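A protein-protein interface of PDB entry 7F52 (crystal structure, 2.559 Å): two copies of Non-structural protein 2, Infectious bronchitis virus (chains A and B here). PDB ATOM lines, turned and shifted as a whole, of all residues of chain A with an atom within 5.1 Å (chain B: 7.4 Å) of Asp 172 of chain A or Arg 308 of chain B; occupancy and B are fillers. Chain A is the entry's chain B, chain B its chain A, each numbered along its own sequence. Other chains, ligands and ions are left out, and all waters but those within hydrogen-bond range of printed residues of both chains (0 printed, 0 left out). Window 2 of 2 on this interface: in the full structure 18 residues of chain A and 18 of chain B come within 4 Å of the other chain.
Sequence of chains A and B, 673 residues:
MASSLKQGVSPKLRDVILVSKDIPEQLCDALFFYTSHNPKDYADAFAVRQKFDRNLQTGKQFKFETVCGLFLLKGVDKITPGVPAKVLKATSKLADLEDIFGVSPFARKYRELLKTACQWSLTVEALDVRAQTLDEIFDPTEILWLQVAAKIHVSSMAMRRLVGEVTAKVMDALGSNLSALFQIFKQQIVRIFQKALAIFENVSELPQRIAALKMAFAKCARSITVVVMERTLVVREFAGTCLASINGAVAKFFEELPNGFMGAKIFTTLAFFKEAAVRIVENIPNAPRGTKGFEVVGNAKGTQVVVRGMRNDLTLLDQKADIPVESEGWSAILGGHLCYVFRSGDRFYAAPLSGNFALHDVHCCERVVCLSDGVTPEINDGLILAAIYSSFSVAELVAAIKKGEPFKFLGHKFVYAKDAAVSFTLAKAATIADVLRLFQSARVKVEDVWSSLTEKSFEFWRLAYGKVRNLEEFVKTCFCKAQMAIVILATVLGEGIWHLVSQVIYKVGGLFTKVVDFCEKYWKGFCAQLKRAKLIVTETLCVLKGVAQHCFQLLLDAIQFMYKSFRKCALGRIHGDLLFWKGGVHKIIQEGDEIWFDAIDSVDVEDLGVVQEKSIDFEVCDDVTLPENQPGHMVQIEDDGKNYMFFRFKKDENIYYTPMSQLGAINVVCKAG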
ATOM      1  N   ALA A 168       5.091  -2.333  -9.982  1.00  0.00           N
ATOM      2  CA  ALA A 168       5.195  -3.789  -9.888  1.00  0.00           C
ATOM      3  C   ALA A 168       6.591  -4.223  -9.396  1.00  0.00           C
ATOM      4  O   ALA A 168       6.722  -5.178  -8.635  1.00  0.00           O
ATOM      5  CB  ALA A 168       4.871  -4.435 -11.237  1.00  0.00           C
ATOM      6  N   LYS A 169       7.630  -3.517  -9.828  1.00  0.00           N
ATOM      7  CA  LYS A 169       8.971  -3.806  -9.342  1.00  0.00           C
ATOM      8  C   LYS A 169       9.086  -3.602  -7.835  1.00  0.00           C
ATOM      9  O   LYS A 169       9.746  -4.394  -7.145  1.00  0.00           O
ATOM     10  CB  LYS A 169      10.011  -2.937 -10.050  1.00  0.00           C
ATOM     11  CG  LYS A 169      10.564  -3.531 -11.344  1.00  0.00           C
ATOM     12  CD  LYS A 169      11.705  -2.666 -11.853  1.00  0.00           C
ATOM     13  CE  LYS A 169      12.060  -2.965 -13.301  1.00  0.00           C
ATOM     14  NZ  LYS A 169      12.740  -1.778 -13.917  1.00  0.00           N
ATOM     15  N   VAL A 170       8.457  -2.543  -7.319  1.00  0.00           N
ATOM     16  CA  VAL A 170       8.511  -2.290  -5.881  1.00  0.00           C
ATOM     17  C   VAL A 170       7.748  -3.394  -5.131  1.00  0.00           C
ATOM     18  O   VAL A 170       8.222  -3.903  -4.133  1.00  0.00           O
ATOM     19  CB  VAL A 170       7.960  -0.885  -5.509  1.00  0.00           C
ATOM     20  CG1 VAL A 170       7.815  -0.735  -3.992  1.00  0.00           C
ATOM     21  CG2 VAL A 170       8.866   0.217  -6.065  1.00  0.00           C
ATOM     22  N   MET A 171       6.588  -3.806  -5.615  1.00  0.00           N
ATOM     23  CA  MET A 171       5.872  -4.875  -4.910  1.00  0.00           C
ATOM     24  C   MET A 171       6.672  -6.191  -4.931  1.00  0.00           C
ATOM     25  O   MET A 171       6.605  -6.960  -3.974  1.00  0.00           O
ATOM     26  CB  MET A 171       4.453  -5.084  -5.490  1.00  0.00           C
ATOM     27  CG  MET A 171       3.532  -3.856  -5.371  1.00  0.00           C
ATOM     28  SD  MET A 171       3.451  -3.038  -3.737  1.00  0.00           S
ATOM     29  CE  MET A 171       3.820  -1.368  -4.246  1.00  0.00           C
ATOM     30  N   ASP A 172       7.426  -6.437  -6.007  1.00  0.00           N
ATOM     31  CA  ASP A 172       8.335  -7.591  -6.078  1.00  0.00           C
ATOM     32  C   ASP A 172       9.470  -7.460  -5.073  1.00  0.00           C
ATOM     33  O   ASP A 172       9.729  -8.370  -4.299  1.00  0.00           O
ATOM     34  CB  ASP A 172       8.959  -7.745  -7.465  1.00  0.00           C
ATOM     35  CG  ASP A 172       8.010  -8.328  -8.478  1.00  0.00           C
ATOM     36  OD1 ASP A 172       6.938  -8.828  -8.080  1.00  0.00           O
ATOM     37  OD2 ASP A 172       8.358  -8.297  -9.679  1.00  0.00           O
ATOM     38  N   ALA A 173      10.152  -6.320  -5.104  1.00  0.00           N
ATOM     39  CA  ALA A 173      11.276  -6.063  -4.210  1.00  0.00           C
ATOM     40  C   ALA A 173      10.879  -6.154  -2.721  1.00  0.00           C
ATOM     41  O   ALA A 173      11.704  -6.450  -1.854  1.00  0.00           O
ATOM     42  CB  ALA A 173      11.888  -4.705  -4.529  1.00  0.00           C
ATOM     43  N   LEU A 174       9.610  -5.928  -2.426  1.00  0.00           N
ATOM     44  CA  LEU A 174       9.148  -5.942  -1.052  1.00  0.00           C
ATOM     45  C   LEU A 174       8.961  -7.357  -0.550  1.00  0.00           C
ATOM     46  O   LEU A 174       9.408  -7.679   0.541  1.00  0.00           O
ATOM     47  CB  LEU A 174       7.841  -5.158  -0.905  1.00  0.00           C
ATOM     48  CG  LEU A 174       7.991  -3.676  -0.571  1.00  0.00           C
ATOM     49  CD1 LEU A 174       6.741  -2.894  -0.977  1.00  0.00           C
ATOM     50  CD2 LEU A 174       8.293  -3.468   0.898  1.00  0.00           C
ATOM     51  N   GLY A 175       8.272  -8.193  -1.316  1.00  0.00           N
ATOM     52  CA  GLY A 175       8.037  -9.563  -0.895  1.00  0.00           C
ATOM     53  C   GLY A 175       6.699  -9.778  -0.215  1.00  0.00           C
ATOM     54  O   GLY A 175       6.134  -8.860   0.378  1.00  0.00           O
ATOM     55  N   SER A 176       6.191 -11.002  -0.299  1.00  0.00           N
ATOM     56  CA  SER A 176       4.908 -11.345   0.310  1.00  0.00           C
ATOM     57  C   SER A 176       4.860 -11.030   1.815  1.00  0.00           C
ATOM     58  O   SER A 176       3.810 -10.660   2.348  1.00  0.00           O
ATOM     59  CB  SER A 176       4.595 -12.822   0.050  1.00  0.00           C
ATOM     60  OG  SER A 176       5.694 -13.634   0.402  1.00  0.00           O
ATOM     61  N   VAL B 305      17.833 -13.366  -0.003  1.00  0.00           N
ATOM     62  CA  VAL B 305      16.832 -13.321  -1.062  1.00  0.00           C
ATOM     63  C   VAL B 305      15.486 -12.754  -0.611  1.00  0.00           C
ATOM     64  O   VAL B 305      15.135 -12.801   0.578  1.00  0.00           O
ATOM     65  CB  VAL B 305      16.585 -14.729  -1.669  1.00  0.00           C
ATOM     66  CG1 VAL B 305      17.851 -15.259  -2.282  1.00  0.00           C
ATOM     67  CG2 VAL B 305      16.034 -15.695  -0.629  1.00  0.00           C
ATOM     68  N   VAL B 306      14.736 -12.227  -1.583  1.00  0.00           N
ATOM     69  CA  VAL B 306      13.373 -11.771  -1.343  1.00  0.00           C
ATOM     70  C   VAL B 306      12.390 -12.810  -1.849  1.00  0.00           C
ATOM     71  O   VAL B 306      12.480 -13.250  -2.987  1.00  0.00           O
ATOM     72  CB  VAL B 306      13.092 -10.429  -2.024  1.00  0.00           C
ATOM     73  CG1 VAL B 306      11.624 -10.065  -1.870  1.00  0.00           C
ATOM     74  CG2 VAL B 306      13.973  -9.354  -1.421  1.00  0.00           C
ATOM     75  N   VAL B 307      11.455 -13.220  -1.003  1.00  0.00           N
ATOM     76  CA  VAL B 307      10.491 -14.238  -1.402  1.00  0.00           C
ATOM     77  C   VAL B 307       9.108 -13.632  -1.784  1.00  0.00           C
ATOM     78  O   VAL B 307       8.496 -12.874  -1.018  1.00  0.00           O
ATOM     79  CB  VAL B 307      10.353 -15.285  -0.275  1.00  0.00           C
ATOM     80  CG1 VAL B 307       9.295 -16.335  -0.629  1.00  0.00           C
ATOM     81  CG2 VAL B 307      11.672 -15.945  -0.055  1.00  0.00           C
ATOM     82  N   ARG B 308       8.634 -13.958  -2.984  1.00  0.00           N
ATOM     83  CA  ARG B 308       7.418 -13.340  -3.541  1.00  0.00           C
ATOM     84  C   ARG B 308       6.159 -14.100  -3.153  1.00  0.00           C
ATOM     85  O   ARG B 308       5.046 -13.580  -3.258  1.00  0.00           O
ATOM     86  CB  ARG B 308       7.490 -13.267  -5.061  1.00  0.00           C
ATOM     87  CG  ARG B 308       8.557 -12.338  -5.607  1.00  0.00           C
ATOM     88  CD  ARG B 308       8.473 -12.288  -7.136  1.00  0.00           C
ATOM     89  NE  ARG B 308       9.534 -11.464  -7.705  1.00  0.00           N
ATOM     90  CZ  ARG B 308       9.749 -11.301  -9.008  1.00  0.00           C
ATOM     91  NH1 ARG B 308       8.972 -11.908  -9.890  1.00  0.00           N
ATOM     92  NH2 ARG B 308      10.746 -10.527  -9.428  1.00  0.00           N
ATOM     93  N   GLY B 309       6.347 -15.345  -2.722  1.00  0.00           N
ATOM     94  CA  GLY B 309       5.249 -16.197  -2.312  1.00  0.00           C
ATOM     95  C   GLY B 309       5.657 -17.659  -2.372  1.00  0.00           C
ATOM     96  O   GLY B 309       6.747 -17.990  -2.830  1.00  0.00           O
ATOM     97  N   MET B 310       4.782 -18.528  -1.883  1.00  0.00           N
ATOM     98  CA  MET B 310       4.920 -19.957  -2.055  1.00  0.00           C
ATOM     99  C   MET B 310       4.386 -20.385  -3.444  1.00  0.00           C
ATOM    100  O   MET B 310       3.357 -19.881  -3.881  1.00  0.00           O
ATOM    101  CB  MET B 310       4.173 -20.670  -0.922  1.00  0.00           C
ATOM    102  CG  MET B 310       4.436 -22.172  -0.831  1.00  0.00           C
ATOM    103  SD  MET B 310       5.795 -22.570   0.292  1.00  0.00           S
ATOM    104  CE  MET B 310       4.912 -22.968   1.804  1.00  0.00           C
ATOM    105  N   ARG B 311       5.094 -21.268  -4.152  1.00  0.00           N
ATOM    106  CA  ARG B 311       4.512 -21.967  -5.318  1.00  0.00           C
ATOM    107  C   ARG B 311       4.673 -23.462  -5.216  1.00  0.00           C
ATOM    108  O   ARG B 311       5.757 -23.943  -4.878  1.00  0.00           O
ATOM    109  CB  ARG B 311       5.288 -21.777  -6.622  1.00  0.00           C
ATOM    110  CG  ARG B 311       6.022 -20.508  -6.812  1.00  0.00           C
ATOM    111  CD  ARG B 311       7.105 -20.694  -7.874  1.00  0.00           C
ATOM    112  NE  ARG B 311       6.528 -20.946  -9.193  1.00  0.00           N
ATOM    113  CZ  ARG B 311       6.645 -20.117 -10.230  1.00  0.00           C
ATOM    114  NH1 ARG B 311       7.330 -18.980 -10.108  1.00  0.00           N
ATOM    115  NH2 ARG B 311       6.088 -20.421 -11.394  1.00  0.00           N
ATOM    116  N   SER B 327      18.460 -12.721  -6.747  1.00  0.00           N
ATOM    117  CA  SER B 327      18.037 -12.220  -5.446  1.00  0.00           C
ATOM    118  C   SER B 327      16.507 -12.172  -5.251  1.00  0.00           C
ATOM    119  O   SER B 327      16.047 -11.891  -4.143  1.00  0.00           O
ATOM    120  CB  SER B 327      18.631 -10.840  -5.200  1.00  0.00           C
ATOM    121  OG  SER B 327      18.237  -9.928  -6.198  1.00  0.00           O
ATOM    122  N   GLU B 328      15.717 -12.461  -6.291  1.00  0.00           N
ATOM    123  CA  GLU B 328      14.262 -12.542  -6.125  1.00  0.00           C
ATOM    124  C   GLU B 328      13.686 -13.845  -6.638  1.00  0.00           C
ATOM    125  O   GLU B 328      14.204 -14.437  -7.581  1.00  0.00           O
ATOM    126  CB  GLU B 328      13.568 -11.390  -6.825  1.00  0.00           C
ATOM    127  CG  GLU B 328      13.853 -10.039  -6.214  1.00  0.00           C
ATOM    128  CD  GLU B 328      13.031  -8.952  -6.867  1.00  0.00           C
ATOM    129  OE1 GLU B 328      12.075  -9.296  -7.604  1.00  0.00           O
ATOM    130  OE2 GLU B 328      13.329  -7.763  -6.624  1.00  0.00           O
ATOM    131  N   GLY B 329      12.590 -14.282  -6.030  1.00  0.00           N
ATOM    132  CA  GLY B 329      12.157 -15.646  -6.210  1.00  0.00           C
ATOM    133  C   GLY B 329      11.017 -16.015  -5.294  1.00  0.00           C
ATOM    134  O   GLY B 329      10.291 -15.155  -4.786  1.00  0.00           O
ATOM    135  N   TRP B 330      10.876 -17.313  -5.085  1.00  0.00           N
ATOM    136  CA  TRP B 330       9.744 -17.894  -4.387  1.00  0.00           C
ATOM    137  C   TRP B 330      10.264 -18.986  -3.467  1.00  0.00           C
ATOM    138  O   TRP B 330      11.363 -19.510  -3.673  1.00  0.00           O
ATOM    139  CB  TRP B 330       8.731 -18.516  -5.368  1.00  0.00           C
ATOM    140  CG  TRP B 330       8.135 -17.578  -6.400  1.00  0.00           C
ATOM    141  CD1 TRP B 330       6.961 -16.876  -6.296  1.00  0.00           C
ATOM    142  CD2 TRP B 330       8.664 -17.276  -7.702  1.00  0.00           C
ATOM    143  NE1 TRP B 330       6.743 -16.142  -7.444  1.00  0.00           N
ATOM    144  CE2 TRP B 330       7.767 -16.373  -8.322  1.00  0.00           C
ATOM    145  CE3 TRP B 330       9.811 -17.673  -8.399  1.00  0.00           C
ATOM    146  CZ2 TRP B 330       7.987 -15.854  -9.592  1.00  0.00           C
ATOM    147  CZ3 TRP B 330      10.016 -17.159  -9.684  1.00  0.00           C
ATOM    148  CH2 TRP B 330       9.107 -16.260 -10.259  1.00  0.00           C
ATOM    149  N   SER B 331       9.463 -19.344  -2.474  1.00  0.00           N
ATOM    150  CA  SER B 331       9.725 -20.507  -1.663  1.00  0.00           C
ATOM    151  C   SER B 331       8.905 -21.696  -2.180  1.00  0.00           C
ATOM    152  O   SER B 331       7.840 -21.510  -2.751  1.00  0.00           O
ATOM    153  CB  SER B 331       9.365 -20.223  -0.220  1.00  0.00           C
ATOM    154  OG  SER B 331       7.953 -20.149  -0.101  1.00  0.00           O
ATOM    155  N   TYR B 340      14.116 -22.582  -1.692  1.00  0.00           N
ATOM    156  CA  TYR B 340      13.989 -21.402  -2.526  1.00  0.00           C
ATOM    157  C   TYR B 340      13.953 -21.845  -3.992  1.00  0.00           C
ATOM    158  O   TYR B 340      14.661 -22.781  -4.380  1.00  0.00           O
ATOM    159  CB  TYR B 340      15.165 -20.490  -2.248  1.00  0.00           C
ATOM    160  CG  TYR B 340      15.218 -19.217  -3.013  1.00  0.00           C
ATOM    161  CD1 TYR B 340      14.286 -18.211  -2.793  1.00  0.00           C
ATOM    162  CD2 TYR B 340      16.240 -18.981  -3.917  1.00  0.00           C
ATOM    163  CE1 TYR B 340      14.363 -17.003  -3.482  1.00  0.00           C
ATOM    164  CE2 TYR B 340      16.324 -17.795  -4.601  1.00  0.00           C
ATOM    165  CZ  TYR B 340      15.386 -16.807  -4.383  1.00  0.00           C
ATOM    166  OH  TYR B 340      15.483 -15.611  -5.048  1.00  0.00           O
ATOM    167  N   ARG B 343      13.850 -18.082 -11.102  1.00  0.00           N
ATOM    168  CA  ARG B 343      13.792 -18.136 -12.537  1.00  0.00           C
ATOM    169  C   ARG B 343      15.006 -17.442 -13.093  1.00  0.00           C
ATOM    170  O   ARG B 343      15.316 -16.306 -12.715  1.00  0.00           O
ATOM    171  CB  ARG B 343      12.509 -17.469 -13.050  1.00  0.00           C
ATOM    172  CG  ARG B 343      12.146 -17.803 -14.489  1.00  0.00           C
ATOM    173  CD  ARG B 343      10.735 -17.314 -14.807  1.00  0.00           C
ATOM    174  NE  ARG B 343      10.179 -17.977 -15.982  1.00  0.00           N
ATOM    175  CZ  ARG B 343      10.068 -17.406 -17.179  1.00  0.00           C
ATOM    176  NH1 ARG B 343      10.470 -16.153 -17.358  1.00  0.00           N
ATOM    177  NH2 ARG B 343       9.553 -18.088 -18.197  1.00  0.00           N
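The guanidinium group of Arg 308 of chain B lies within salt-bridge range of the side-chain carboxylate of Asp 172 of chain A (3.3 Å). O of Val 307 of chain B sits at hydrogen-bond distance from N of Ser 176 of chain A, at 3.1 Å.
O of Gly 309 of chain B sits at hydrogen-bond distance from N of Ser 331 of chain B (3.1 Å). The guanidinium group of Arg 308 of chain B lies within salt-bridge range of the side-chain carboxylate of Glu 328 of chain B (2.6 Å). The backbone carbonyl oxygen of Val 306 of chain B sits at hydrogen-bond distance from the backbone NH of Gly 329 of chain B, at 3.2 Å. N of Val 306 of chain B lies within hydrogen-bond range of O of Ser 327 of chain B. The backbone carbonyl oxygen (O) of Glu 328 of chain B lies close to the side-chain hydroxyl (OH) of Tyr 340 of chain B (3.1 Å). O of Gly 329 of chain B lies within hydrogen-bond range of N of Arg 308 of chain B (2.7 Å).
Asp 172 of chain A touches Val 306 of chain B (O to CG1, 3.5 Å). Asp 172 of chain A touches Glu 328 of chain B (CB to OE1, 3.5 Å). Val 306 of chain B touches Ala 173 of chain A. Ala 173 of chain A touches Glu 328 of chain B (CA to OE2, 3.6 Å). Gly 175 of chain A touches Val 306 of chain B. Gly 175 of chain A touches Val 307 of chain B. CB of Ser 176 of chain A touches O of Arg 308 of chain B, 3.4 Å away. Gly 309 of chain B touches Ser 176 of chain A (N to OG, 3.6 Å).
Of chain B, only Val 306, Arg 308 and Glu 328 come within 4 Å of Asp 172 of chain A. Printed residues of chain B within 4 Å of Ala 173 of chain A: Val 306 (3.6 Å) and Glu 328 (3.6 Å). Printed residues of chain A within 4 Å of Val 307 of chain B: Gly 175 and Ser 176. Of the printed residues of chain A, Arg 308 of chain B touches Asp 172 (3.3 Å) and Ser 176 (3.4 Å). Printed residues of chain A within 4 Å of Gly 309 of chain B: Ser 176 (3.6 Å). Arg 311 of chain B touches none of the printed residues of chain A. Ser 327 of chain B touches none of the printed residues of chain A.
Of the 9 printed residues of chain A, 4 touch a printed residue of chain B. Hydrophobic or aromatic side chains of chain A that line the printed part of chain B: Ala 173. Along chain A the printed residues that touch a printed residue of chain B span positions 172 to 176. Printed residues of chain B that touch a printed residue of chain A: Val 306, Val 307, Arg 308, Gly 309 and Glu 328. Among the printed residues, 10 pairs touch across the chains.
No position is printed for both chains.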
